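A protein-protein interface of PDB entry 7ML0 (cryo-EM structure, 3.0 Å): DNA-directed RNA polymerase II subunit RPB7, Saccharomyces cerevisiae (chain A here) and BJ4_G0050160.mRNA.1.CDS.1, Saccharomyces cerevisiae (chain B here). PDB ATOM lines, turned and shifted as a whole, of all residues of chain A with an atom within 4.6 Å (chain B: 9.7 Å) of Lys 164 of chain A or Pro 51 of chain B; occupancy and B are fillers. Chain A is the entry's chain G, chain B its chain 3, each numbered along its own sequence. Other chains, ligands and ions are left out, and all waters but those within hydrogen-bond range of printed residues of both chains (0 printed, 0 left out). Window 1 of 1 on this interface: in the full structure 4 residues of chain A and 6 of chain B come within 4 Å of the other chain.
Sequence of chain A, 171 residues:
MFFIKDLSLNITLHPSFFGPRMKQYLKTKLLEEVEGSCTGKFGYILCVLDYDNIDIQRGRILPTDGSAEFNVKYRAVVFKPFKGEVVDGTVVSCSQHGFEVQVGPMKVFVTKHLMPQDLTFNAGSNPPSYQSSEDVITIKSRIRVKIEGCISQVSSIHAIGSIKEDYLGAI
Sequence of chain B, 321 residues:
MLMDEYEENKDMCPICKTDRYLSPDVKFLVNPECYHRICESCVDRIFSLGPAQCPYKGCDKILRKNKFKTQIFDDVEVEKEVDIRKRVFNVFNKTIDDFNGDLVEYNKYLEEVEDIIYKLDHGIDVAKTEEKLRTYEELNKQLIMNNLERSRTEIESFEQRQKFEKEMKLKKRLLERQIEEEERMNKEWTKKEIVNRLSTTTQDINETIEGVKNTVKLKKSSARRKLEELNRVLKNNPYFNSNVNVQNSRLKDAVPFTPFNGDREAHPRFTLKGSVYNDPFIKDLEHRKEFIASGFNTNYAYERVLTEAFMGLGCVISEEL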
ATOM      1  N   HIS A 113     -16.086  -6.821   6.407  1.00  0.00           N
ATOM      2  CA  HIS A 113     -15.184  -5.718   6.126  1.00  0.00           C
ATOM      3  C   HIS A 113     -15.824  -4.676   5.229  1.00  0.00           C
ATOM      4  O   HIS A 113     -15.282  -3.577   5.084  1.00  0.00           O
ATOM      5  CB  HIS A 113     -13.924  -6.269   5.475  1.00  0.00           C
ATOM      6  CG  HIS A 113     -13.306  -7.411   6.225  1.00  0.00           C
ATOM      7  ND1 HIS A 113     -14.022  -8.513   6.640  1.00  0.00           N
ATOM      8  CD2 HIS A 113     -12.030  -7.624   6.619  1.00  0.00           C
ATOM      9  CE1 HIS A 113     -13.217  -9.353   7.260  1.00  0.00           C
ATOM     10  NE2 HIS A 113     -12.002  -8.837   7.263  1.00  0.00           N
ATOM     11  N   LEU A 114     -16.967  -5.005   4.649  1.00  0.00           N
ATOM     12  CA  LEU A 114     -17.823  -4.111   3.896  1.00  0.00           C
ATOM     13  C   LEU A 114     -19.112  -3.782   4.627  1.00  0.00           C
ATOM     14  O   LEU A 114     -19.730  -2.756   4.347  1.00  0.00           O
ATOM     15  CB  LEU A 114     -18.168  -4.742   2.546  1.00  0.00           C
ATOM     16  CG  LEU A 114     -17.012  -5.088   1.610  1.00  0.00           C
ATOM     17  CD1 LEU A 114     -16.328  -6.386   1.981  1.00  0.00           C
ATOM     18  CD2 LEU A 114     -17.533  -5.155   0.193  1.00  0.00           C
ATOM     19  N   MET A 115     -19.529  -4.639   5.546  1.00  0.00           N
ATOM     20  CA  MET A 115     -20.697  -4.417   6.362  1.00  0.00           C
ATOM     21  C   MET A 115     -20.335  -3.515   7.543  1.00  0.00           C
ATOM     22  O   MET A 115     -19.152  -3.308   7.829  1.00  0.00           O
ATOM     23  CB  MET A 115     -21.219  -5.774   6.822  1.00  0.00           C
ATOM     24  CG  MET A 115     -21.379  -6.756   5.680  1.00  0.00           C
ATOM     25  SD  MET A 115     -21.468  -8.474   6.211  1.00  0.00           S
ATOM     26  CE  MET A 115     -21.848  -8.272   7.946  1.00  0.00           C
ATOM     27  N   PRO A 116     -21.330  -2.957   8.245  1.00  0.00           N
ATOM     28  CA  PRO A 116     -21.020  -1.979   9.294  1.00  0.00           C
ATOM     29  C   PRO A 116     -20.189  -2.590  10.415  1.00  0.00           C
ATOM     30  O   PRO A 116     -20.441  -3.710  10.864  1.00  0.00           O
ATOM     31  CB  PRO A 116     -22.402  -1.546   9.785  1.00  0.00           C
ATOM     32  CG  PRO A 116     -23.256  -2.722   9.532  1.00  0.00           C
ATOM     33  CD  PRO A 116     -22.767  -3.290   8.245  1.00  0.00           C
ATOM     34  N   GLN A 117     -19.211  -1.816  10.892  1.00  0.00           N
ATOM     35  CA  GLN A 117     -18.174  -2.358  11.766  1.00  0.00           C
ATOM     36  C   GLN A 117     -18.705  -2.811  13.114  1.00  0.00           C
ATOM     37  O   GLN A 117     -18.015  -3.552  13.819  1.00  0.00           O
ATOM     38  CB  GLN A 117     -17.072  -1.320  11.981  1.00  0.00           C
ATOM     39  CG  GLN A 117     -17.423   0.074  11.492  1.00  0.00           C
ATOM     40  CD  GLN A 117     -18.078   0.916  12.555  1.00  0.00           C
ATOM     41  OE1 GLN A 117     -18.978   0.462  13.255  1.00  0.00           O
ATOM     42  NE2 GLN A 117     -17.624   2.155  12.689  1.00  0.00           N
ATOM     43  N   SER A 162     -22.378  -5.265   0.325  1.00  0.00           N
ATOM     44  CA  SER A 162     -22.149  -4.668   1.631  1.00  0.00           C
ATOM     45  C   SER A 162     -23.477  -4.183   2.181  1.00  0.00           C
ATOM     46  O   SER A 162     -24.407  -3.891   1.427  1.00  0.00           O
ATOM     47  CB  SER A 162     -21.185  -3.489   1.558  1.00  0.00           C
ATOM     48  OG  SER A 162     -21.875  -2.339   1.104  1.00  0.00           O
ATOM     49  N   ILE A 163     -23.551  -4.082   3.508  1.00  0.00           N
ATOM     50  CA  ILE A 163     -24.736  -3.553   4.174  1.00  0.00           C
ATOM     51  C   ILE A 163     -24.341  -2.455   5.142  1.00  0.00           C
ATOM     52  O   ILE A 163     -25.014  -2.241   6.153  1.00  0.00           O
ATOM     53  CB  ILE A 163     -25.512  -4.655   4.911  1.00  0.00           C
ATOM     54  CG1 ILE A 163     -24.571  -5.473   5.790  1.00  0.00           C
ATOM     55  CG2 ILE A 163     -26.275  -5.504   3.928  1.00  0.00           C
ATOM     56  CD1 ILE A 163     -25.083  -6.838   6.135  1.00  0.00           C
ATOM     57  N   LYS A 164     -23.254  -1.749   4.847  1.00  0.00           N
ATOM     58  CA  LYS A 164     -22.690  -0.852   5.842  1.00  0.00           C
ATOM     59  C   LYS A 164     -23.633   0.276   6.231  1.00  0.00           C
ATOM     60  O   LYS A 164     -23.482   0.845   7.313  1.00  0.00           O
ATOM     61  CB  LYS A 164     -21.366  -0.276   5.349  1.00  0.00           C
ATOM     62  CG  LYS A 164     -20.262  -0.414   6.378  1.00  0.00           C
ATOM     63  CD  LYS A 164     -19.097   0.497   6.129  1.00  0.00           C
ATOM     64  CE  LYS A 164     -18.294   0.013   4.969  1.00  0.00           C
ATOM     65  NZ  LYS A 164     -17.543  -1.208   5.296  1.00  0.00           N
ATOM     66  N   GLU A 165     -24.603   0.604   5.402  1.00  0.00           N
ATOM     67  CA  GLU A 165     -25.386   1.812   5.602  1.00  0.00           C
ATOM     68  C   GLU A 165     -26.776   1.480   6.135  1.00  0.00           C
ATOM     69  O   GLU A 165     -27.062   0.356   6.555  1.00  0.00           O
ATOM     70  CB  GLU A 165     -25.438   2.626   4.308  1.00  0.00           C
ATOM     71  CG  GLU A 165     -24.067   3.069   3.792  1.00  0.00           C
ATOM     72  CD  GLU A 165     -23.195   1.900   3.352  1.00  0.00           C
ATOM     73  OE1 GLU A 165     -23.728   0.790   3.143  1.00  0.00           O
ATOM     74  OE2 GLU A 165     -21.971   2.079   3.239  1.00  0.00           O
ATOM     75  N   ASP A 166     -27.638   2.483   6.155  1.00  0.00           N
ATOM     76  CA  ASP A 166     -28.980   2.349   6.685  1.00  0.00           C
ATOM     77  C   ASP A 166     -29.876   1.569   5.721  1.00  0.00           C
ATOM     78  O   ASP A 166     -29.579   1.420   4.533  1.00  0.00           O
ATOM     79  CB  ASP A 166     -29.564   3.728   6.957  1.00  0.00           C
ATOM     80  CG  ASP A 166     -29.482   4.625   5.756  1.00  0.00           C
ATOM     81  OD1 ASP A 166     -29.031   4.139   4.701  1.00  0.00           O
ATOM     82  OD2 ASP A 166     -29.865   5.807   5.861  1.00  0.00           O
ATOM     83  N   LEU A 168     -30.081  -1.380   5.809  1.00  0.00           N
ATOM     84  CA  LEU A 168     -29.282  -2.525   5.408  1.00  0.00           C
ATOM     85  C   LEU A 168     -29.111  -3.483   6.573  1.00  0.00           C
ATOM     86  O   LEU A 168     -29.750  -3.318   7.614  1.00  0.00           O
ATOM     87  CB  LEU A 168     -27.936  -2.057   4.869  1.00  0.00           C
ATOM     88  CG  LEU A 168     -28.072  -1.100   3.678  1.00  0.00           C
ATOM     89  CD1 LEU A 168     -26.718  -0.636   3.162  1.00  0.00           C
ATOM     90  CD2 LEU A 168     -28.900  -1.720   2.559  1.00  0.00           C
ATOM     91  N   VAL B  43     -12.700  12.741   1.574  1.00  0.00           N
ATOM     92  CA  VAL B  43     -14.133  12.564   1.803  1.00  0.00           C
ATOM     93  C   VAL B  43     -14.634  11.315   1.105  1.00  0.00           C
ATOM     94  O   VAL B  43     -15.232  10.431   1.729  1.00  0.00           O
ATOM     95  CB  VAL B  43     -14.931  13.782   1.312  1.00  0.00           C
ATOM     96  CG1 VAL B  43     -16.410  13.431   1.219  1.00  0.00           C
ATOM     97  CG2 VAL B  43     -14.703  14.971   2.224  1.00  0.00           C
ATOM     98  N   ASP B  44     -14.397  11.245  -0.199  1.00  0.00           N
ATOM     99  CA  ASP B  44     -14.795  10.069  -0.951  1.00  0.00           C
ATOM    100  C   ASP B  44     -14.087   8.833  -0.428  1.00  0.00           C
ATOM    101  O   ASP B  44     -14.734   7.863  -0.026  1.00  0.00           O
ATOM    102  CB  ASP B  44     -14.491  10.301  -2.423  1.00  0.00           C
ATOM    103  CG  ASP B  44     -14.533  11.764  -2.780  1.00  0.00           C
ATOM    104  OD1 ASP B  44     -15.354  12.486  -2.181  1.00  0.00           O
ATOM    105  OD2 ASP B  44     -13.731  12.200  -3.628  1.00  0.00           O
ATOM    106  N   ARG B  45     -12.753   8.880  -0.356  1.00  0.00           N
ATOM    107  CA  ARG B  45     -11.989   7.720   0.098  1.00  0.00           C
ATOM    108  C   ARG B  45     -12.451   7.271   1.475  1.00  0.00           C
ATOM    109  O   ARG B  45     -12.581   6.072   1.743  1.00  0.00           O
ATOM    110  CB  ARG B  45     -10.491   8.035   0.116  1.00  0.00           C
ATOM    111  CG  ARG B  45      -9.617   6.868   0.586  1.00  0.00           C
ATOM    112  CD  ARG B  45      -9.154   7.035   2.032  1.00  0.00           C
ATOM    113  NE  ARG B  45      -9.555   5.918   2.887  1.00  0.00           N
ATOM    114  CZ  ARG B  45      -8.856   4.796   3.038  1.00  0.00           C
ATOM    115  NH1 ARG B  45      -7.713   4.632   2.388  1.00  0.00           N
ATOM    116  NH2 ARG B  45      -9.295   3.835   3.838  1.00  0.00           N
ATOM    117  N   ILE B  46     -12.715   8.232   2.357  1.00  0.00           N
ATOM    118  CA  ILE B  46     -13.140   7.902   3.709  1.00  0.00           C
ATOM    119  C   ILE B  46     -14.493   7.203   3.702  1.00  0.00           C
ATOM    120  O   ILE B  46     -14.684   6.189   4.383  1.00  0.00           O
ATOM    121  CB  ILE B  46     -13.155   9.168   4.584  1.00  0.00           C
ATOM    122  CG1 ILE B  46     -11.745   9.456   5.097  1.00  0.00           C
ATOM    123  CG2 ILE B  46     -14.126   9.013   5.750  1.00  0.00           C
ATOM    124  CD1 ILE B  46     -11.209   8.369   6.010  1.00  0.00           C
ATOM    125  N   PHE B  47     -15.457   7.727   2.942  1.00  0.00           N
ATOM    126  CA  PHE B  47     -16.818   7.208   3.003  1.00  0.00           C
ATOM    127  C   PHE B  47     -17.344   6.722   1.661  1.00  0.00           C
ATOM    128  O   PHE B  47     -18.559   6.580   1.492  1.00  0.00           O
ATOM    129  CB  PHE B  47     -17.749   8.252   3.597  1.00  0.00           C
ATOM    130  CG  PHE B  47     -17.542   8.445   5.050  1.00  0.00           C
ATOM    131  CD1 PHE B  47     -17.231   7.364   5.852  1.00  0.00           C
ATOM    132  CD2 PHE B  47     -17.618   9.690   5.615  1.00  0.00           C
ATOM    133  CE1 PHE B  47     -17.020   7.520   7.186  1.00  0.00           C
ATOM    134  CE2 PHE B  47     -17.401   9.850   6.950  1.00  0.00           C
ATOM    135  CZ  PHE B  47     -17.096   8.756   7.734  1.00  0.00           C
ATOM    136  N   SER B  48     -16.460   6.446   0.706  1.00  0.00           N
ATOM    137  CA  SER B  48     -16.863   5.583  -0.391  1.00  0.00           C
ATOM    138  C   SER B  48     -17.201   4.184   0.093  1.00  0.00           C
ATOM    139  O   SER B  48     -17.954   3.479  -0.584  1.00  0.00           O
ATOM    140  CB  SER B  48     -15.761   5.509  -1.441  1.00  0.00           C
ATOM    141  OG  SER B  48     -14.495   5.424  -0.808  1.00  0.00           O
ATOM    142  N   LEU B  49     -16.684   3.778   1.252  1.00  0.00           N
ATOM    143  CA  LEU B  49     -16.942   2.445   1.782  1.00  0.00           C
ATOM    144  C   LEU B  49     -18.199   2.425   2.641  1.00  0.00           C
ATOM    145  O   LEU B  49     -19.073   1.578   2.422  1.00  0.00           O
ATOM    146  CB  LEU B  49     -15.721   1.936   2.564  1.00  0.00           C
ATOM    147  CG  LEU B  49     -15.224   2.760   3.754  1.00  0.00           C
ATOM    148  CD1 LEU B  49     -15.306   1.952   5.041  1.00  0.00           C
ATOM    149  CD2 LEU B  49     -13.807   3.278   3.528  1.00  0.00           C
ATOM    150  N   GLY B  50     -18.338   3.344   3.590  1.00  0.00           N
ATOM    151  CA  GLY B  50     -19.539   3.413   4.381  1.00  0.00           C
ATOM    152  C   GLY B  50     -19.343   3.992   5.763  1.00  0.00           C
ATOM    153  O   GLY B  50     -18.284   4.530   6.101  1.00  0.00           O
ATOM    154  N   PRO B  51     -20.378   3.878   6.594  1.00  0.00           N
ATOM    155  CA  PRO B  51     -20.399   4.590   7.878  1.00  0.00           C
ATOM    156  C   PRO B  51     -19.245   4.218   8.785  1.00  0.00           C
ATOM    157  O   PRO B  51     -19.147   3.081   9.260  1.00  0.00           O
ATOM    158  CB  PRO B  51     -21.737   4.164   8.490  1.00  0.00           C
ATOM    159  CG  PRO B  51     -22.563   3.760   7.334  1.00  0.00           C
ATOM    160  CD  PRO B  51     -21.623   3.137   6.357  1.00  0.00           C
ATOM    161  N   ALA B  52     -18.360   5.178   9.024  1.00  0.00           N
ATOM    162  CA  ALA B  52     -17.217   4.982   9.897  1.00  0.00           C
ATOM    163  C   ALA B  52     -16.876   6.298  10.581  1.00  0.00           C
ATOM    164  O   ALA B  52     -17.587   7.300  10.456  1.00  0.00           O
ATOM    165  CB  ALA B  52     -16.018   4.423   9.120  1.00  0.00           C
ATOM    166  N   GLN B  53     -15.772   6.282  11.304  1.00  0.00           N
ATOM    167  CA  GLN B  53     -15.311   7.427  12.064  1.00  0.00           C
ATOM    168  C   GLN B  53     -14.834   8.537  11.135  1.00  0.00           C
ATOM    169  O   GLN B  53     -14.423   8.289   9.998  1.00  0.00           O
ATOM    170  CB  GLN B  53     -14.183   6.994  12.996  1.00  0.00           C
ATOM    171  CG  GLN B  53     -13.131   6.151  12.292  1.00  0.00           C
ATOM    172  CD  GLN B  53     -12.765   4.894  13.059  1.00  0.00           C
ATOM    173  OE1 GLN B  53     -13.611   4.276  13.707  1.00  0.00           O
ATOM    174  NE2 GLN B  53     -11.494   4.514  12.996  1.00  0.00           N
ATOM    175  N   CYS B  54     -14.903   9.769  11.625  1.00  0.00           N
ATOM    176  CA  CYS B  54     -14.333  10.886  10.889  1.00  0.00           C
ATOM    177  C   CYS B  54     -12.812  10.790  10.918  1.00  0.00           C
ATOM    178  O   CYS B  54     -12.237  10.486  11.972  1.00  0.00           O
ATOM    179  CB  CYS B  54     -14.779  12.220  11.480  1.00  0.00           C
ATOM    180  SG  CYS B  54     -13.982  13.661  10.723  1.00  0.00           S
ATOM    181  N   ASP B  60     -14.252  10.372  16.862  1.00  0.00           N
ATOM    182  CA  ASP B  60     -14.859   9.060  16.682  1.00  0.00           C
ATOM    183  C   ASP B  60     -16.346   9.210  16.410  1.00  0.00           C
ATOM    184  O   ASP B  60     -17.147   8.364  16.810  1.00  0.00           O
ATOM    185  CB  ASP B  60     -14.621   8.165  17.895  1.00  0.00           C
ATOM    186  CG  ASP B  60     -13.205   7.651  17.967  1.00  0.00           C
ATOM    187  OD1 ASP B  60     -12.566   7.515  16.904  1.00  0.00           O
ATOM    188  OD2 ASP B  60     -12.727   7.385  19.087  1.00  0.00           O
ATOM    189  N   LYS B  61     -16.725  10.295  15.743  1.00  0.00           N
ATOM    190  CA  LYS B  61     -18.100  10.516  15.326  1.00  0.00           C
ATOM    191  C   LYS B  61     -18.348   9.727  14.054  1.00  0.00           C
ATOM    192  O   LYS B  61     -17.832  10.084  12.995  1.00  0.00           O
ATOM    193  CB  LYS B  61     -18.367  11.999  15.091  1.00  0.00           C
ATOM    194  CG  LYS B  61     -18.319  12.819  16.353  1.00  0.00           C
ATOM    195  CD  LYS B  61     -18.483  14.291  16.061  1.00  0.00           C
ATOM    196  CE  LYS B  61     -18.577  15.088  17.350  1.00  0.00           C
ATOM    197  NZ  LYS B  61     -17.434  14.809  18.263  1.00  0.00           N
ATOM    198  N   ILE B  62     -19.109   8.642  14.163  1.00  0.00           N
ATOM    199  CA  ILE B  62     -19.419   7.859  12.983  1.00  0.00           C
ATOM    200  C   ILE B  62     -20.421   8.615  12.125  1.00  0.00           C
ATOM    201  O   ILE B  62     -21.502   9.009  12.582  1.00  0.00           O
ATOM    202  CB  ILE B  62     -19.947   6.470  13.374  1.00  0.00           C
ATOM    203  CG1 ILE B  62     -18.967   5.800  14.342  1.00  0.00           C
ATOM    204  CG2 ILE B  62     -20.154   5.625  12.128  1.00  0.00           C
ATOM    205  CD1 ILE B  62     -19.458   4.500  14.906  1.00  0.00           C
ATOM    206  N   LEU B  63     -20.065   8.806  10.862  1.00  0.00           N
ATOM    207  CA  LEU B  63     -20.799   9.698   9.985  1.00  0.00           C
ATOM    208  C   LEU B  63     -20.674   9.175   8.563  1.00  0.00           C
ATOM    209  O   LEU B  63     -19.863   8.294   8.280  1.00  0.00           O
ATOM    210  CB  LEU B  63     -20.301  11.142  10.121  1.00  0.00           C
ATOM    211  CG  LEU B  63     -18.927  11.612   9.636  1.00  0.00           C
ATOM    212  CD1 LEU B  63     -18.702  13.038  10.050  1.00  0.00           C
ATOM    213  CD2 LEU B  63     -17.812  10.790  10.186  1.00  0.00           C
ATOM    214  N   ARG B  64     -21.529   9.681   7.682  1.00  0.00           N
ATOM    215  CA  ARG B  64     -21.755   9.057   6.389  1.00  0.00           C
ATOM    216  C   ARG B  64     -21.765  10.094   5.274  1.00  0.00           C
ATOM    217  O   ARG B  64     -22.216  11.228   5.458  1.00  0.00           O
ATOM    218  CB  ARG B  64     -23.068   8.272   6.399  1.00  0.00           C
ATOM    219  CG  ARG B  64     -23.209   7.313   7.578  1.00  0.00           C
ATOM    220  CD  ARG B  64     -24.637   7.268   8.084  1.00  0.00           C
ATOM    221  NE  ARG B  64     -25.323   6.029   7.741  1.00  0.00           N
ATOM    222  CZ  ARG B  64     -25.445   4.994   8.562  1.00  0.00           C
ATOM    223  NH1 ARG B  64     -24.918   5.045   9.774  1.00  0.00           N
ATOM    224  NH2 ARG B  64     -26.092   3.909   8.171  1.00  0.00           N
ATOM    225  N   LYS B  65     -21.284   9.669   4.100  1.00  0.00           N
ATOM    226  CA  LYS B  65     -20.953  10.609   3.031  1.00  0.00           C
ATOM    227  C   LYS B  65     -22.186  11.339   2.511  1.00  0.00           C
ATOM    228  O   LYS B  65     -22.082  12.472   2.024  1.00  0.00           O
ATOM    229  CB  LYS B  65     -20.241   9.876   1.893  1.00  0.00           C
ATOM    230  CG  LYS B  65     -19.477  10.797   0.953  1.00  0.00           C
ATOM    231  CD  LYS B  65     -18.162  10.184   0.470  1.00  0.00           C
ATOM    232  CE  LYS B  65     -18.390   9.006  -0.460  1.00  0.00           C
ATOM    233  NZ  LYS B  65     -19.262   9.342  -1.607  1.00  0.00           N
ATOM    234  N   ASN B  66     -23.356  10.711   2.588  1.00  0.00           N
ATOM    235  CA  ASN B  66     -24.554  11.431   2.179  1.00  0.00           C
ATOM    236  C   ASN B  66     -24.866  12.601   3.090  1.00  0.00           C
ATOM    237  O   ASN B  66     -25.431  13.597   2.624  1.00  0.00           O
ATOM    238  CB  ASN B  66     -25.761  10.494   2.138  1.00  0.00           C
ATOM    239  CG  ASN B  66     -27.057  11.234   1.852  1.00  0.00           C
ATOM    240  OD1 ASN B  66     -27.318  11.638   0.718  1.00  0.00           O
ATOM    241  ND2 ASN B  66     -27.870  11.426   2.881  1.00  0.00           N
ATOM    242  N   LYS B  67     -24.489  12.528   4.359  1.00  0.00           N
ATOM    243  CA  LYS B  67     -24.745  13.608   5.293  1.00  0.00           C
ATOM    244  C   LYS B  67     -23.795  14.769   5.077  1.00  0.00           C
ATOM    245  O   LYS B  67     -23.955  15.819   5.704  1.00  0.00           O
ATOM    246  CB  LYS B  67     -24.642  13.098   6.728  1.00  0.00           C
ATOM    247  CG  LYS B  67     -25.281  11.741   6.947  1.00  0.00           C
ATOM    248  CD  LYS B  67     -26.733  11.737   6.528  1.00  0.00           C
ATOM    249  CE  LYS B  67     -27.288  10.333   6.521  1.00  0.00           C
ATOM    250  NZ  LYS B  67     -27.310   9.757   7.882  1.00  0.00           N
ATOM    251  N   PHE B  68     -22.820  14.607   4.195  1.00  0.00           N
ATOM    252  CA  PHE B  68     -21.807  15.618   3.969  1.00  0.00           C
ATOM    253  C   PHE B  68     -22.401  16.806   3.238  1.00  0.00           C
ATOM    254  O   PHE B  68     -23.479  16.721   2.644  1.00  0.00           O
ATOM    255  CB  PHE B  68     -20.633  15.029   3.192  1.00  0.00           C
ATOM    256  CG  PHE B  68     -19.661  14.295   4.061  1.00  0.00           C
ATOM    257  CD1 PHE B  68     -18.316  14.601   4.031  1.00  0.00           C
ATOM    258  CD2 PHE B  68     -20.102  13.325   4.941  1.00  0.00           C
ATOM    259  CE1 PHE B  68     -17.428  13.930   4.847  1.00  0.00           C
ATOM    260  CE2 PHE B  68     -19.227  12.657   5.758  1.00  0.00           C
ATOM    261  CZ  PHE B  68     -17.887  12.960   5.714  1.00  0.00           C
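O of Leu 49 of chain B sits close to OE2 of Glu 165 of chain A (3.1 Å).
NH2 of Arg 64 of chain B sits close to N of Asp 166 of chain A (2.9 Å).
The backbone carbonyl oxygen (O) of Ala 52 of chain B sits at hydrogen-bond distance from the backbone NH (N) of Leu 63 of chain B, at 2.9 Å.
The backbone carbonyl oxygen (O) of His 113 of chain A lies within hydrogen-bond range of the side-chain amino group (NZ) of Lys 164 of chain A (3.3 Å).
The side-chain amino group of Lys 164 of chain A is in hydrogen-bond range of the backbone carbonyl oxygen of Leu 114 of chain A (2.8 Å).
NE2 of Gln 117 of chain A touches O of Pro 51 of chain B, 3.9 Å away.
Gln 117 of chain A touches Ala 52 of chain B.
Ile 62 of chain B touches Gln 117 of chain A (CD1 to NE2, 3.7 Å).
Leu 49 of chain B touches Lys 164 of chain A.
Gly 50 of chain B touches Lys 164 of chain A.
CG of Pro 51 of chain B touches O of Lys 164 of chain A, at 3.1 Å.
CA of Gly 50 of chain B touches OE2 of Glu 165 of chain A, at 3.0 Å.
Pro 51 of chain B touches Glu 165 of chain A.
Arg 64 of chain B touches Glu 165 of chain A.
Lys 164 of chain A touches just these residues of chain B: Leu 49 (3.1 Å), Gly 50 (3.4 Å) and Pro 51 (3.1 Å).
Of chain A, only Gln 117, Lys 164 and Glu 165 come within 4 Å of Pro 51 of chain B.
No residue of chain B comes within 4 Å of Ile 163 of chain A.
Glu 165 of chain A touches just these residues of chain B: Leu 49, Gly 50, Pro 51 and Arg 64.
Printed residues of chain A within 4 Å of Ala 52 of chain B: Gln 117.
Of the printed residues of chain A, Ile 62 of chain B touches Gln 117 (3.7 Å).
The nearest residue of chain B that does not touch Lys 164 of chain A is Arg 64 of chain B (4.1 Å).
The nearest printed residue of chain A that does not touch Pro 51 of chain B is Asp 166 of chain A (5.4 Å).
The nearest printed residue of chain A that does not touch Gly 50 of chain B is Leu 114 of chain A (6.2 Å).
Of the 21 printed residues of chain B, 6 touch a printed residue of chain A.
Among the printed residues, 11 pairs touch across the chains.
Among the printed residues, no Asp or Glu carboxylate lies within 4 Å of a Lys or Arg side-chain nitrogen of the other chain.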
